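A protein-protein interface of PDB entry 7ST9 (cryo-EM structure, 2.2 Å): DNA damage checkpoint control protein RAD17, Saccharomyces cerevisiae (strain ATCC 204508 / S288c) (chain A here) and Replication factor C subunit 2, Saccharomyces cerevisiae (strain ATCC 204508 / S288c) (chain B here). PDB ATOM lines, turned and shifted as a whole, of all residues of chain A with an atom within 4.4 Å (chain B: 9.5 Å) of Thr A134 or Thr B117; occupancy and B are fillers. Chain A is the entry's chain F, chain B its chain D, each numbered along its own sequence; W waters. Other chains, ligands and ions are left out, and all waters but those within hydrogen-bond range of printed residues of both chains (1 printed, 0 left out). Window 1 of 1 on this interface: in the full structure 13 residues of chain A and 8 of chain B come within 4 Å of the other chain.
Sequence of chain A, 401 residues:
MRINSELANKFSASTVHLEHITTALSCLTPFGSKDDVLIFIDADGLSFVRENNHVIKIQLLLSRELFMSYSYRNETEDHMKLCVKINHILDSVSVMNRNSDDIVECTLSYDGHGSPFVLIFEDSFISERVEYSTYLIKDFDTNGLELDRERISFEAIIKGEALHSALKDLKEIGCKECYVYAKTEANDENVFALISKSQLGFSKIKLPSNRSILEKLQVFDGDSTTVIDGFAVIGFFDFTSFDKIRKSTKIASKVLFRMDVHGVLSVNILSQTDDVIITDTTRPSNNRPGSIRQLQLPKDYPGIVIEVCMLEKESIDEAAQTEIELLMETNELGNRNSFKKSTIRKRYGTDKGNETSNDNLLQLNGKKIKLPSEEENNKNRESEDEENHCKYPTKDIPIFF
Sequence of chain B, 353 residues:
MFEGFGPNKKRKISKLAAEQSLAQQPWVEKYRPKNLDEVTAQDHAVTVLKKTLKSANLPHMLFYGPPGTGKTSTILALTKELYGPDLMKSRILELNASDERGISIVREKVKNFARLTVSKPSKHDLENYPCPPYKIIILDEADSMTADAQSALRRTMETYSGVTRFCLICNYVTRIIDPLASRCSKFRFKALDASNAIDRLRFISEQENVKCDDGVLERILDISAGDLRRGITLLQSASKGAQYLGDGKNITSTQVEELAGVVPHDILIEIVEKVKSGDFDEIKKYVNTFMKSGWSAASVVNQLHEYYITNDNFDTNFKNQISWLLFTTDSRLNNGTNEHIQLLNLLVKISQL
The backbone carbonyl oxygen (O) of Leu B116 lies within hydrogen-bond range of the side-chain amino group (NZ) of Lys B135, 2.5 Å away. The backbone NH (N) of Lys B135 is in hydrogen-bond range of the backbone carbonyl oxygen (O) of Val B163, 2.8 Å away. The backbone NH (N) of Tyr A135 sits at hydrogen-bond distance from the backbone carbonyl oxygen (O) of Cys A83.
Water W1 lies within hydrogen-bond range of a ring nitrogen (ND1) of His A113 (2.6 Å) and the backbone carbonyl oxygen (O) of Val B118 (3.1 Å).
His A113 touches Thr B117. Ser A115 touches Lys B120 (OG to CE, 3.8 Å). Ser A133 touches Leu B116 (CB to CD1, 3.8 Å). Thr A134 touches Leu B116 (O to CD1, 3.6 Å). Tyr A135 touches Asn B112. CA of Tyr A135 touches O of Arg B115 (3.5 Å). CE2 of Tyr A135 touches CD1 of Leu B116, at 3.5 Å. Thr B117 touches Tyr A135. N of Leu A136 touches CG2 of Thr B117 (3.8 Å). Val B163 touches Leu A136 (CG2 to CD1, 3.6 Å).
The guanidinium group (NH2) of Arg B115 sits at hydrogen-bond distance from the side-chain sulfur (SG) of Cys A83 (3.6 Å). O of Arg B115 is in hydrogen-bond range of N of Leu A136. OG1 of Thr B117 sits at hydrogen-bond distance from OG1 of Thr A134 (2.6 Å). The side-chain amino group of Lys B120 sits close to the backbone carbonyl oxygen of His A113.
Hydrophobic or aromatic side chains of chain A that line the printed part of chain B: His A113, Tyr A135 and Leu A136. Printed residues of chain B that touch a printed residue of chain A: Asn B112, Arg B115, Leu B116, Thr B117, Lys B120 and Val B163. Among the printed residues, no Asp or Glu carboxylate lies within 4 Å of a Lys or Arg side-chain nitrogen of the other chain.
Of chain B, only Leu B116 (3.6 Å) and Thr B117 (2.6 Å) come within 4 Å of Thr A134. Of chain B, only Leu B116 (3.8 Å) comes within 4 Å of Ser A133. Printed residues of chain B within 4 Å of Ser A115: Lys B120 (3.8 Å). Of the printed residues of chain B, Tyr A135 touches Asn B112 (3.4 Å), Arg B115 (3.5 Å), Leu B116 (3.5 Å) and Thr B117 (3.5 Å). Leu B87 touches none of the printed residues of chain A. The nearest printed residue of chain B that does not touch His A113 is Val B118 (5.1 Å).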
ATOM      1  N   LEU A  82      31.985  -4.919 -32.143  1.00  0.00           N
ATOM      2  CA  LEU A  82      30.592  -4.586 -32.418  1.00  0.00           C
ATOM      3  C   LEU A  82      29.769  -5.865 -32.470  1.00  0.00           C
ATOM      4  O   LEU A  82      30.304  -6.971 -32.525  1.00  0.00           O
ATOM      5  CB  LEU A  82      30.446  -3.779 -33.717  1.00  0.00           C
ATOM      6  CG  LEU A  82      30.837  -4.460 -35.027  1.00  0.00           C
ATOM      7  CD1 LEU A  82      29.968  -3.956 -36.168  1.00  0.00           C
ATOM      8  CD2 LEU A  82      32.309  -4.227 -35.330  1.00  0.00           C
ATOM      9  N   CYS A  83      28.449  -5.702 -32.431  1.00  0.00           N
ATOM     10  CA  CYS A  83      27.520  -6.824 -32.443  1.00  0.00           C
ATOM     11  C   CYS A  83      26.414  -6.549 -33.449  1.00  0.00           C
ATOM     12  O   CYS A  83      25.867  -5.443 -33.486  1.00  0.00           O
ATOM     13  CB  CYS A  83      26.927  -7.057 -31.051  1.00  0.00           C
ATOM     14  SG  CYS A  83      25.864  -8.502 -30.936  1.00  0.00           S
ATOM     15  N   HIS A 113      32.157   3.169 -32.350  1.00  0.00           N
ATOM     16  CA  HIS A 113      30.924   2.930 -31.612  1.00  0.00           C
ATOM     17  C   HIS A 113      29.884   3.990 -31.948  1.00  0.00           C
ATOM     18  O   HIS A 113      30.202   5.170 -32.114  1.00  0.00           O
ATOM     19  CB  HIS A 113      31.204   2.925 -30.109  1.00  0.00           C
ATOM     20  CG  HIS A 113      30.238   2.102 -29.317  1.00  0.00           C
ATOM     21  ND1 HIS A 113      29.499   2.619 -28.274  1.00  0.00           N
ATOM     22  CD2 HIS A 113      29.889   0.797 -29.412  1.00  0.00           C
ATOM     23  CE1 HIS A 113      28.736   1.669 -27.763  1.00  0.00           C
ATOM     24  NE2 HIS A 113      28.954   0.553 -28.435  1.00  0.00           N
ATOM     25  N   SER A 115      28.047   3.968 -34.719  1.00  0.00           N
ATOM     26  CA  SER A 115      27.835   4.001 -36.156  1.00  0.00           C
ATOM     27  C   SER A 115      27.462   2.615 -36.670  1.00  0.00           C
ATOM     28  O   SER A 115      27.803   1.604 -36.049  1.00  0.00           O
ATOM     29  CB  SER A 115      29.089   4.488 -36.892  1.00  0.00           C
ATOM     30  OG  SER A 115      30.253   3.855 -36.391  1.00  0.00           O
ATOM     31  N   PHE A 117      27.389  -0.770 -39.225  1.00  0.00           N
ATOM     32  CA  PHE A 117      28.334  -1.559 -40.006  1.00  0.00           C
ATOM     33  C   PHE A 117      27.896  -1.513 -41.464  1.00  0.00           C
ATOM     34  O   PHE A 117      26.786  -1.944 -41.793  1.00  0.00           O
ATOM     35  CB  PHE A 117      28.383  -2.996 -39.491  1.00  0.00           C
ATOM     36  CG  PHE A 117      29.496  -3.814 -40.079  1.00  0.00           C
ATOM     37  CD1 PHE A 117      30.819  -3.507 -39.806  1.00  0.00           C
ATOM     38  CD2 PHE A 117      29.219  -4.892 -40.901  1.00  0.00           C
ATOM     39  CE1 PHE A 117      31.844  -4.259 -40.344  1.00  0.00           C
ATOM     40  CE2 PHE A 117      30.240  -5.648 -41.442  1.00  0.00           C
ATOM     41  CZ  PHE A 117      31.554  -5.331 -41.163  1.00  0.00           C
ATOM     42  N   TYR A 132      23.961  -1.890 -41.195  1.00  0.00           N
ATOM     43  CA  TYR A 132      23.454  -2.756 -40.141  1.00  0.00           C
ATOM     44  C   TYR A 132      23.594  -2.053 -38.799  1.00  0.00           C
ATOM     45  O   TYR A 132      24.686  -1.591 -38.446  1.00  0.00           O
ATOM     46  CB  TYR A 132      24.209  -4.085 -40.110  1.00  0.00           C
ATOM     47  CG  TYR A 132      24.157  -4.865 -41.402  1.00  0.00           C
ATOM     48  CD1 TYR A 132      22.983  -5.470 -41.825  1.00  0.00           C
ATOM     49  CD2 TYR A 132      25.288  -5.005 -42.193  1.00  0.00           C
ATOM     50  CE1 TYR A 132      22.936  -6.188 -43.003  1.00  0.00           C
ATOM     51  CE2 TYR A 132      25.251  -5.720 -43.370  1.00  0.00           C
ATOM     52  CZ  TYR A 132      24.074  -6.310 -43.771  1.00  0.00           C
ATOM     53  OH  TYR A 132      24.037  -7.022 -44.945  1.00  0.00           O
ATOM     54  N   SER A 133      22.491  -1.973 -38.062  1.00  0.00           N
ATOM     55  CA  SER A 133      22.525  -1.417 -36.719  1.00  0.00           C
ATOM     56  C   SER A 133      23.291  -2.343 -35.781  1.00  0.00           C
ATOM     57  O   SER A 133      23.277  -3.568 -35.932  1.00  0.00           O
ATOM     58  CB  SER A 133      21.106  -1.200 -36.197  1.00  0.00           C
ATOM     59  OG  SER A 133      20.329  -0.464 -37.123  1.00  0.00           O
ATOM     60  N   THR A 134      23.967  -1.744 -34.806  1.00  0.00           N
ATOM     61  CA  THR A 134      24.764  -2.475 -33.833  1.00  0.00           C
ATOM     62  C   THR A 134      24.069  -2.480 -32.477  1.00  0.00           C
ATOM     63  O   THR A 134      23.235  -1.622 -32.175  1.00  0.00           O
ATOM     64  CB  THR A 134      26.164  -1.866 -33.702  1.00  0.00           C
ATOM     65  OG1 THR A 134      26.063  -0.518 -33.225  1.00  0.00           O
ATOM     66  CG2 THR A 134      26.879  -1.877 -35.045  1.00  0.00           C
ATOM     67  N   TYR A 135      24.428  -3.466 -31.659  1.00  0.00           N
ATOM     68  CA  TYR A 135      23.808  -3.674 -30.360  1.00  0.00           C
ATOM     69  C   TYR A 135      24.881  -3.855 -29.297  1.00  0.00           C
ATOM     70  O   TYR A 135      26.032  -4.185 -29.593  1.00  0.00           O
ATOM     71  CB  TYR A 135      22.874  -4.892 -30.376  1.00  0.00           C
ATOM     72  CG  TYR A 135      21.781  -4.799 -31.413  1.00  0.00           C
ATOM     73  CD1 TYR A 135      22.024  -5.128 -32.740  1.00  0.00           C
ATOM     74  CD2 TYR A 135      20.504  -4.375 -31.068  1.00  0.00           C
ATOM     75  CE1 TYR A 135      21.030  -5.039 -33.693  1.00  0.00           C
ATOM     76  CE2 TYR A 135      19.502  -4.286 -32.013  1.00  0.00           C
ATOM     77  CZ  TYR A 135      19.770  -4.619 -33.323  1.00  0.00           C
ATOM     78  OH  TYR A 135      18.774  -4.530 -34.267  1.00  0.00           O
ATOM     79  N   LEU A 136      24.487  -3.628 -28.047  1.00  0.00           N
ATOM     80  CA  LEU A 136      25.403  -3.816 -26.931  1.00  0.00           C
ATOM     81  C   LEU A 136      25.841  -5.272 -26.847  1.00  0.00           C
ATOM     82  O   LEU A 136      25.062  -6.192 -27.110  1.00  0.00           O
ATOM     83  CB  LEU A 136      24.738  -3.391 -25.621  1.00  0.00           C
ATOM     84  CG  LEU A 136      24.509  -1.893 -25.401  1.00  0.00           C
ATOM     85  CD1 LEU A 136      24.056  -1.635 -23.972  1.00  0.00           C
ATOM     86  CD2 LEU A 136      25.758  -1.079 -25.717  1.00  0.00           C
ATOM     87  N   LEU B  87      17.932  14.180 -34.351  1.00  0.00           N
ATOM     88  CA  LEU B  87      18.393  13.069 -33.526  1.00  0.00           C
ATOM     89  C   LEU B  87      17.231  12.254 -32.969  1.00  0.00           C
ATOM     90  O   LEU B  87      17.358  11.035 -32.804  1.00  0.00           O
ATOM     91  CB  LEU B  87      19.270  13.600 -32.392  1.00  0.00           C
ATOM     92  CG  LEU B  87      20.023  12.566 -31.552  1.00  0.00           C
ATOM     93  CD1 LEU B  87      20.988  11.759 -32.408  1.00  0.00           C
ATOM     94  CD2 LEU B  87      20.761  13.252 -30.415  1.00  0.00           C
ATOM     95  N   SER B  90      16.198   8.761 -34.216  1.00  0.00           N
ATOM     96  CA  SER B  90      17.016   7.600 -33.899  1.00  0.00           C
ATOM     97  C   SER B  90      17.121   7.321 -32.406  1.00  0.00           C
ATOM     98  O   SER B  90      17.706   6.299 -32.028  1.00  0.00           O
ATOM     99  CB  SER B  90      18.428   7.774 -34.478  1.00  0.00           C
ATOM    100  OG  SER B  90      19.028   8.968 -34.009  1.00  0.00           O
ATOM    101  N   ARG B  91      16.574   8.187 -31.552  1.00  0.00           N
ATOM    102  CA  ARG B  91      16.682   8.024 -30.109  1.00  0.00           C
ATOM    103  C   ARG B  91      15.345   7.780 -29.422  1.00  0.00           C
ATOM    104  O   ARG B  91      15.320   7.624 -28.196  1.00  0.00           O
ATOM    105  CB  ARG B  91      17.345   9.260 -29.483  1.00  0.00           C
ATOM    106  CG  ARG B  91      18.756   9.537 -29.977  1.00  0.00           C
ATOM    107  CD  ARG B  91      19.721   8.432 -29.580  1.00  0.00           C
ATOM    108  NE  ARG B  91      21.113   8.843 -29.736  1.00  0.00           N
ATOM    109  CZ  ARG B  91      21.782   9.580 -28.860  1.00  0.00           C
ATOM    110  NH1 ARG B  91      21.223  10.003 -27.738  1.00  0.00           N
ATOM    111  NH2 ARG B  91      23.047   9.902 -29.117  1.00  0.00           N
ATOM    112  N   LYS B 111      12.777  -5.081 -26.664  1.00  0.00           N
ATOM    113  CA  LYS B 111      14.080  -5.536 -26.190  1.00  0.00           C
ATOM    114  C   LYS B 111      15.184  -5.181 -27.178  1.00  0.00           C
ATOM    115  O   LYS B 111      16.268  -4.742 -26.775  1.00  0.00           O
ATOM    116  CB  LYS B 111      14.048  -7.044 -25.941  1.00  0.00           C
ATOM    117  CG  LYS B 111      15.134  -7.534 -24.998  1.00  0.00           C
ATOM    118  CD  LYS B 111      14.973  -9.014 -24.691  1.00  0.00           C
ATOM    119  CE  LYS B 111      15.999  -9.488 -23.677  1.00  0.00           C
ATOM    120  NZ  LYS B 111      15.835 -10.932 -23.355  1.00  0.00           N
ATOM    121  N   ASN B 112      14.934  -5.365 -28.478  1.00  0.00           N
ATOM    122  CA  ASN B 112      15.943  -5.033 -29.476  1.00  0.00           C
ATOM    123  C   ASN B 112      16.261  -3.546 -29.460  1.00  0.00           C
ATOM    124  O   ASN B 112      17.433  -3.156 -29.506  1.00  0.00           O
ATOM    125  CB  ASN B 112      15.468  -5.460 -30.864  1.00  0.00           C
ATOM    126  CG  ASN B 112      15.445  -6.966 -31.033  1.00  0.00           C
ATOM    127  OD1 ASN B 112      16.095  -7.695 -30.287  1.00  0.00           O
ATOM    128  ND2 ASN B 112      14.692  -7.437 -32.020  1.00  0.00           N
ATOM    129  N   PHE B 113      15.232  -2.698 -29.393  1.00  0.00           N
ATOM    130  CA  PHE B 113      15.485  -1.262 -29.360  1.00  0.00           C
ATOM    131  C   PHE B 113      16.232  -0.863 -28.093  1.00  0.00           C
ATOM    132  O   PHE B 113      17.154  -0.042 -28.139  1.00  0.00           O
ATOM    133  CB  PHE B 113      14.176  -0.484 -29.473  1.00  0.00           C
ATOM    134  CG  PHE B 113      14.372   0.992 -29.674  1.00  0.00           C
ATOM    135  CD1 PHE B 113      14.625   1.505 -30.935  1.00  0.00           C
ATOM    136  CD2 PHE B 113      14.318   1.864 -28.601  1.00  0.00           C
ATOM    137  CE1 PHE B 113      14.810   2.861 -31.123  1.00  0.00           C
ATOM    138  CE2 PHE B 113      14.503   3.222 -28.783  1.00  0.00           C
ATOM    139  CZ  PHE B 113      14.749   3.720 -30.045  1.00  0.00           C
ATOM    140  N   ALA B 114      15.849  -1.438 -26.949  1.00  0.00           N
ATOM    141  CA  ALA B 114      16.516  -1.102 -25.696  1.00  0.00           C
ATOM    142  C   ALA B 114      17.986  -1.498 -25.722  1.00  0.00           C
ATOM    143  O   ALA B 114      18.815  -0.849 -25.075  1.00  0.00           O
ATOM    144  CB  ALA B 114      15.805  -1.780 -24.525  1.00  0.00           C
ATOM    145  N   ARG B 115      18.325  -2.557 -26.454  1.00  0.00           N
ATOM    146  CA  ARG B 115      19.702  -3.016 -26.574  1.00  0.00           C
ATOM    147  C   ARG B 115      20.479  -2.297 -27.669  1.00  0.00           C
ATOM    148  O   ARG B 115      21.690  -2.506 -27.786  1.00  0.00           O
ATOM    149  CB  ARG B 115      19.721  -4.523 -26.849  1.00  0.00           C
ATOM    150  CG  ARG B 115      21.018  -5.207 -26.471  1.00  0.00           C
ATOM    151  CD  ARG B 115      20.923  -6.704 -26.682  1.00  0.00           C
ATOM    152  NE  ARG B 115      22.196  -7.274 -27.104  1.00  0.00           N
ATOM    153  CZ  ARG B 115      22.324  -8.336 -27.887  1.00  0.00           C
ATOM    154  NH1 ARG B 115      21.270  -8.978 -28.365  1.00  0.00           N
ATOM    155  NH2 ARG B 115      23.543  -8.768 -28.197  1.00  0.00           N
ATOM    156  N   LEU B 116      19.818  -1.461 -28.466  1.00  0.00           N
ATOM    157  CA  LEU B 116      20.488  -0.779 -29.565  1.00  0.00           C
ATOM    158  C   LEU B 116      21.571   0.156 -29.040  1.00  0.00           C
ATOM    159  O   LEU B 116      21.399   0.821 -28.016  1.00  0.00           O
ATOM    160  CB  LEU B 116      19.469   0.010 -30.387  1.00  0.00           C
ATOM    161  CG  LEU B 116      19.856   0.331 -31.830  1.00  0.00           C
ATOM    162  CD1 LEU B 116      19.722  -0.903 -32.707  1.00  0.00           C
ATOM    163  CD2 LEU B 116      19.005   1.471 -32.366  1.00  0.00           C
ATOM    164  N   THR B 117      22.693   0.207 -29.752  1.00  0.00           N
ATOM    165  CA  THR B 117      23.758   1.131 -29.394  1.00  0.00           C
ATOM    166  C   THR B 117      23.300   2.572 -29.600  1.00  0.00           C
ATOM    167  O   THR B 117      22.510   2.875 -30.498  1.00  0.00           O
ATOM    168  CB  THR B 117      25.015   0.862 -30.225  1.00  0.00           C
ATOM    169  OG1 THR B 117      24.702   0.950 -31.621  1.00  0.00           O
ATOM    170  CG2 THR B 117      25.577  -0.517 -29.918  1.00  0.00           C
ATOM    171  N   VAL B 118      23.806   3.464 -28.750  1.00  0.00           N
ATOM    172  CA  VAL B 118      23.433   4.871 -28.832  1.00  0.00           C
ATOM    173  C   VAL B 118      24.002   5.465 -30.113  1.00  0.00           C
ATOM    174  O   VAL B 118      25.204   5.360 -30.388  1.00  0.00           O
ATOM    175  CB  VAL B 118      23.928   5.630 -27.592  1.00  0.00           C
ATOM    176  CG1 VAL B 118      23.491   7.085 -27.646  1.00  0.00           C
ATOM    177  CG2 VAL B 118      23.417   4.962 -26.320  1.00  0.00           C
ATOM    178  N   SER B 119      23.136   6.092 -30.905  1.00  0.00           N
ATOM    179  CA  SER B 119      23.551   6.632 -32.192  1.00  0.00           C
ATOM    180  C   SER B 119      24.458   7.843 -32.007  1.00  0.00           C
ATOM    181  O   SER B 119      24.336   8.601 -31.041  1.00  0.00           O
ATOM    182  CB  SER B 119      22.328   7.016 -33.025  1.00  0.00           C
ATOM    183  OG  SER B 119      21.687   8.165 -32.499  1.00  0.00           O
ATOM    184  N   LYS B 120      25.373   8.020 -32.950  1.00  0.00           N
ATOM    185  CA  LYS B 120      26.327   9.121 -32.887  1.00  0.00           C
ATOM    186  C   LYS B 120      25.628  10.442 -33.185  1.00  0.00           C
ATOM    187  O   LYS B 120      25.048  10.591 -34.268  1.00  0.00           O
ATOM    188  CB  LYS B 120      27.459   8.897 -33.887  1.00  0.00           C
ATOM    189  CG  LYS B 120      28.625   8.081 -33.353  1.00  0.00           C
ATOM    190  CD  LYS B 120      29.884   8.326 -34.178  1.00  0.00           C
ATOM    191  CE  LYS B 120      30.669   7.044 -34.413  1.00  0.00           C
ATOM    192  NZ  LYS B 120      31.501   6.672 -33.235  1.00  0.00           N
ATOM    193  N   PRO B 121      25.646  11.415 -32.276  1.00  0.00           N
ATOM    194  CA  PRO B 121      25.121  12.740 -32.622  1.00  0.00           C
ATOM    195  C   PRO B 121      26.031  13.452 -33.609  1.00  0.00           C
ATOM    196  O   PRO B 121      27.243  13.228 -33.649  1.00  0.00           O
ATOM    197  CB  PRO B 121      25.074  13.476 -31.276  1.00  0.00           C
ATOM    198  CG  PRO B 121      25.270  12.428 -30.228  1.00  0.00           C
ATOM    199  CD  PRO B 121      26.069  11.347 -30.868  1.00  0.00           C
ATOM    200  N   PRO B 133      23.418  10.587 -23.589  1.00  0.00           N
ATOM    201  CA  PRO B 133      23.875   9.324 -24.184  1.00  0.00           C
ATOM    202  C   PRO B 133      22.967   8.125 -23.904  1.00  0.00           C
ATOM    203  O   PRO B 133      23.419   7.073 -23.450  1.00  0.00           O
ATOM    204  CB  PRO B 133      25.259   9.142 -23.555  1.00  0.00           C
ATOM    205  CG  PRO B 133      25.112   9.735 -22.196  1.00  0.00           C
ATOM    206  CD  PRO B 133      24.117  10.869 -22.321  1.00  0.00           C
ATOM    207  N   TYR B 134      21.675   8.283 -24.180  1.00  0.00           N
ATOM    208  CA  TYR B 134      20.744   7.168 -24.066  1.00  0.00           C
ATOM    209  C   TYR B 134      19.524   7.447 -24.930  1.00  0.00           C
ATOM    210  O   TYR B 134      19.277   8.582 -25.343  1.00  0.00           O
ATOM    211  CB  TYR B 134      20.331   6.917 -22.609  1.00  0.00           C
ATOM    212  CG  TYR B 134      19.948   8.159 -21.837  1.00  0.00           C
ATOM    213  CD1 TYR B 134      18.772   8.842 -22.118  1.00  0.00           C
ATOM    214  CD2 TYR B 134      20.756   8.641 -20.817  1.00  0.00           C
ATOM    215  CE1 TYR B 134      18.419   9.975 -21.413  1.00  0.00           C
ATOM    216  CE2 TYR B 134      20.411   9.771 -20.105  1.00  0.00           C
ATOM    217  CZ  TYR B 134      19.242  10.434 -20.406  1.00  0.00           C
ATOM    218  OH  TYR B 134      18.895  11.562 -19.699  1.00  0.00           O
ATOM    219  N   LYS B 135      18.770   6.387 -25.202  1.00  0.00           N
ATOM    220  CA  LYS B 135      17.524   6.465 -25.948  1.00  0.00           C
ATOM    221  C   LYS B 135      16.342   6.520 -24.985  1.00  0.00           C
ATOM    222  O   LYS B 135      16.492   6.385 -23.769  1.00  0.00           O
ATOM    223  CB  LYS B 135      17.378   5.269 -26.896  1.00  0.00           C
ATOM    224  CG  LYS B 135      18.638   4.886 -27.662  1.00  0.00           C
ATOM    225  CD  LYS B 135      18.688   3.388 -27.915  1.00  0.00           C
ATOM    226  CE  LYS B 135      19.181   2.639 -26.686  1.00  0.00           C
ATOM    227  NZ  LYS B 135      19.216   1.168 -26.897  1.00  0.00           N
ATOM    228  N   TYR B 160      19.311  -2.599 -19.234  1.00  0.00           N
ATOM    229  CA  TYR B 160      19.771  -1.647 -20.237  1.00  0.00           C
ATOM    230  C   TYR B 160      19.513  -0.201 -19.824  1.00  0.00           C
ATOM    231  O   TYR B 160      19.404   0.684 -20.677  1.00  0.00           O
ATOM    232  CB  TYR B 160      19.112  -1.946 -21.583  1.00  0.00           C
ATOM    233  CG  TYR B 160      19.351  -3.362 -22.053  1.00  0.00           C
ATOM    234  CD1 TYR B 160      20.624  -3.789 -22.405  1.00  0.00           C
ATOM    235  CD2 TYR B 160      18.309  -4.275 -22.130  1.00  0.00           C
ATOM    236  CE1 TYR B 160      20.851  -5.083 -22.828  1.00  0.00           C
ATOM    237  CE2 TYR B 160      18.526  -5.572 -22.553  1.00  0.00           C
ATOM    238  CZ  TYR B 160      19.800  -5.970 -22.901  1.00  0.00           C
ATOM    239  OH  TYR B 160      20.024  -7.259 -23.324  1.00  0.00           O
ATOM    240  N   GLY B 162      21.532   1.796 -18.696  1.00  0.00           N
ATOM    241  CA  GLY B 162      22.672   2.625 -19.044  1.00  0.00           C
ATOM    242  C   GLY B 162      22.564   3.286 -20.402  1.00  0.00           C
ATOM    243  O   GLY B 162      23.222   4.306 -20.634  1.00  0.00           O
ATOM    244  N   VAL B 163      21.753   2.732 -21.305  1.00  0.00           N
ATOM    245  CA  VAL B 163      21.585   3.281 -22.644  1.00  0.00           C
ATOM    246  C   VAL B 163      20.128   3.525 -23.004  1.00  0.00           C
ATOM    247  O   VAL B 163      19.853   4.074 -24.072  1.00  0.00           O
ATOM    248  CB  VAL B 163      22.243   2.374 -23.705  1.00  0.00           C
ATOM    249  CG1 VAL B 163      23.740   2.266 -23.458  1.00  0.00           C
ATOM    250  CG2 VAL B 163      21.593   0.993 -23.715  1.00  0.00           C
ATOM    251  N   THR B 164      19.181   3.137 -22.151  1.00  0.00           N
ATOM    252  CA  THR B 164      17.764   3.278 -22.452  1.00  0.00           C
ATOM    253  C   THR B 164      17.008   3.695 -21.200  1.00  0.00           C
ATOM    254  O   THR B 164      17.322   3.246 -20.095  1.00  0.00           O
ATOM    255  CB  THR B 164      17.173   1.968 -22.993  1.00  0.00           C
ATOM    256  OG1 THR B 164      18.027   1.440 -24.014  1.00  0.00           O
ATOM    257  CG2 THR B 164      15.783   2.199 -23.565  1.00  0.00           C
HETATM  258  O   HOH W   1      27.666   4.421 -28.785  1.00  0.00           O
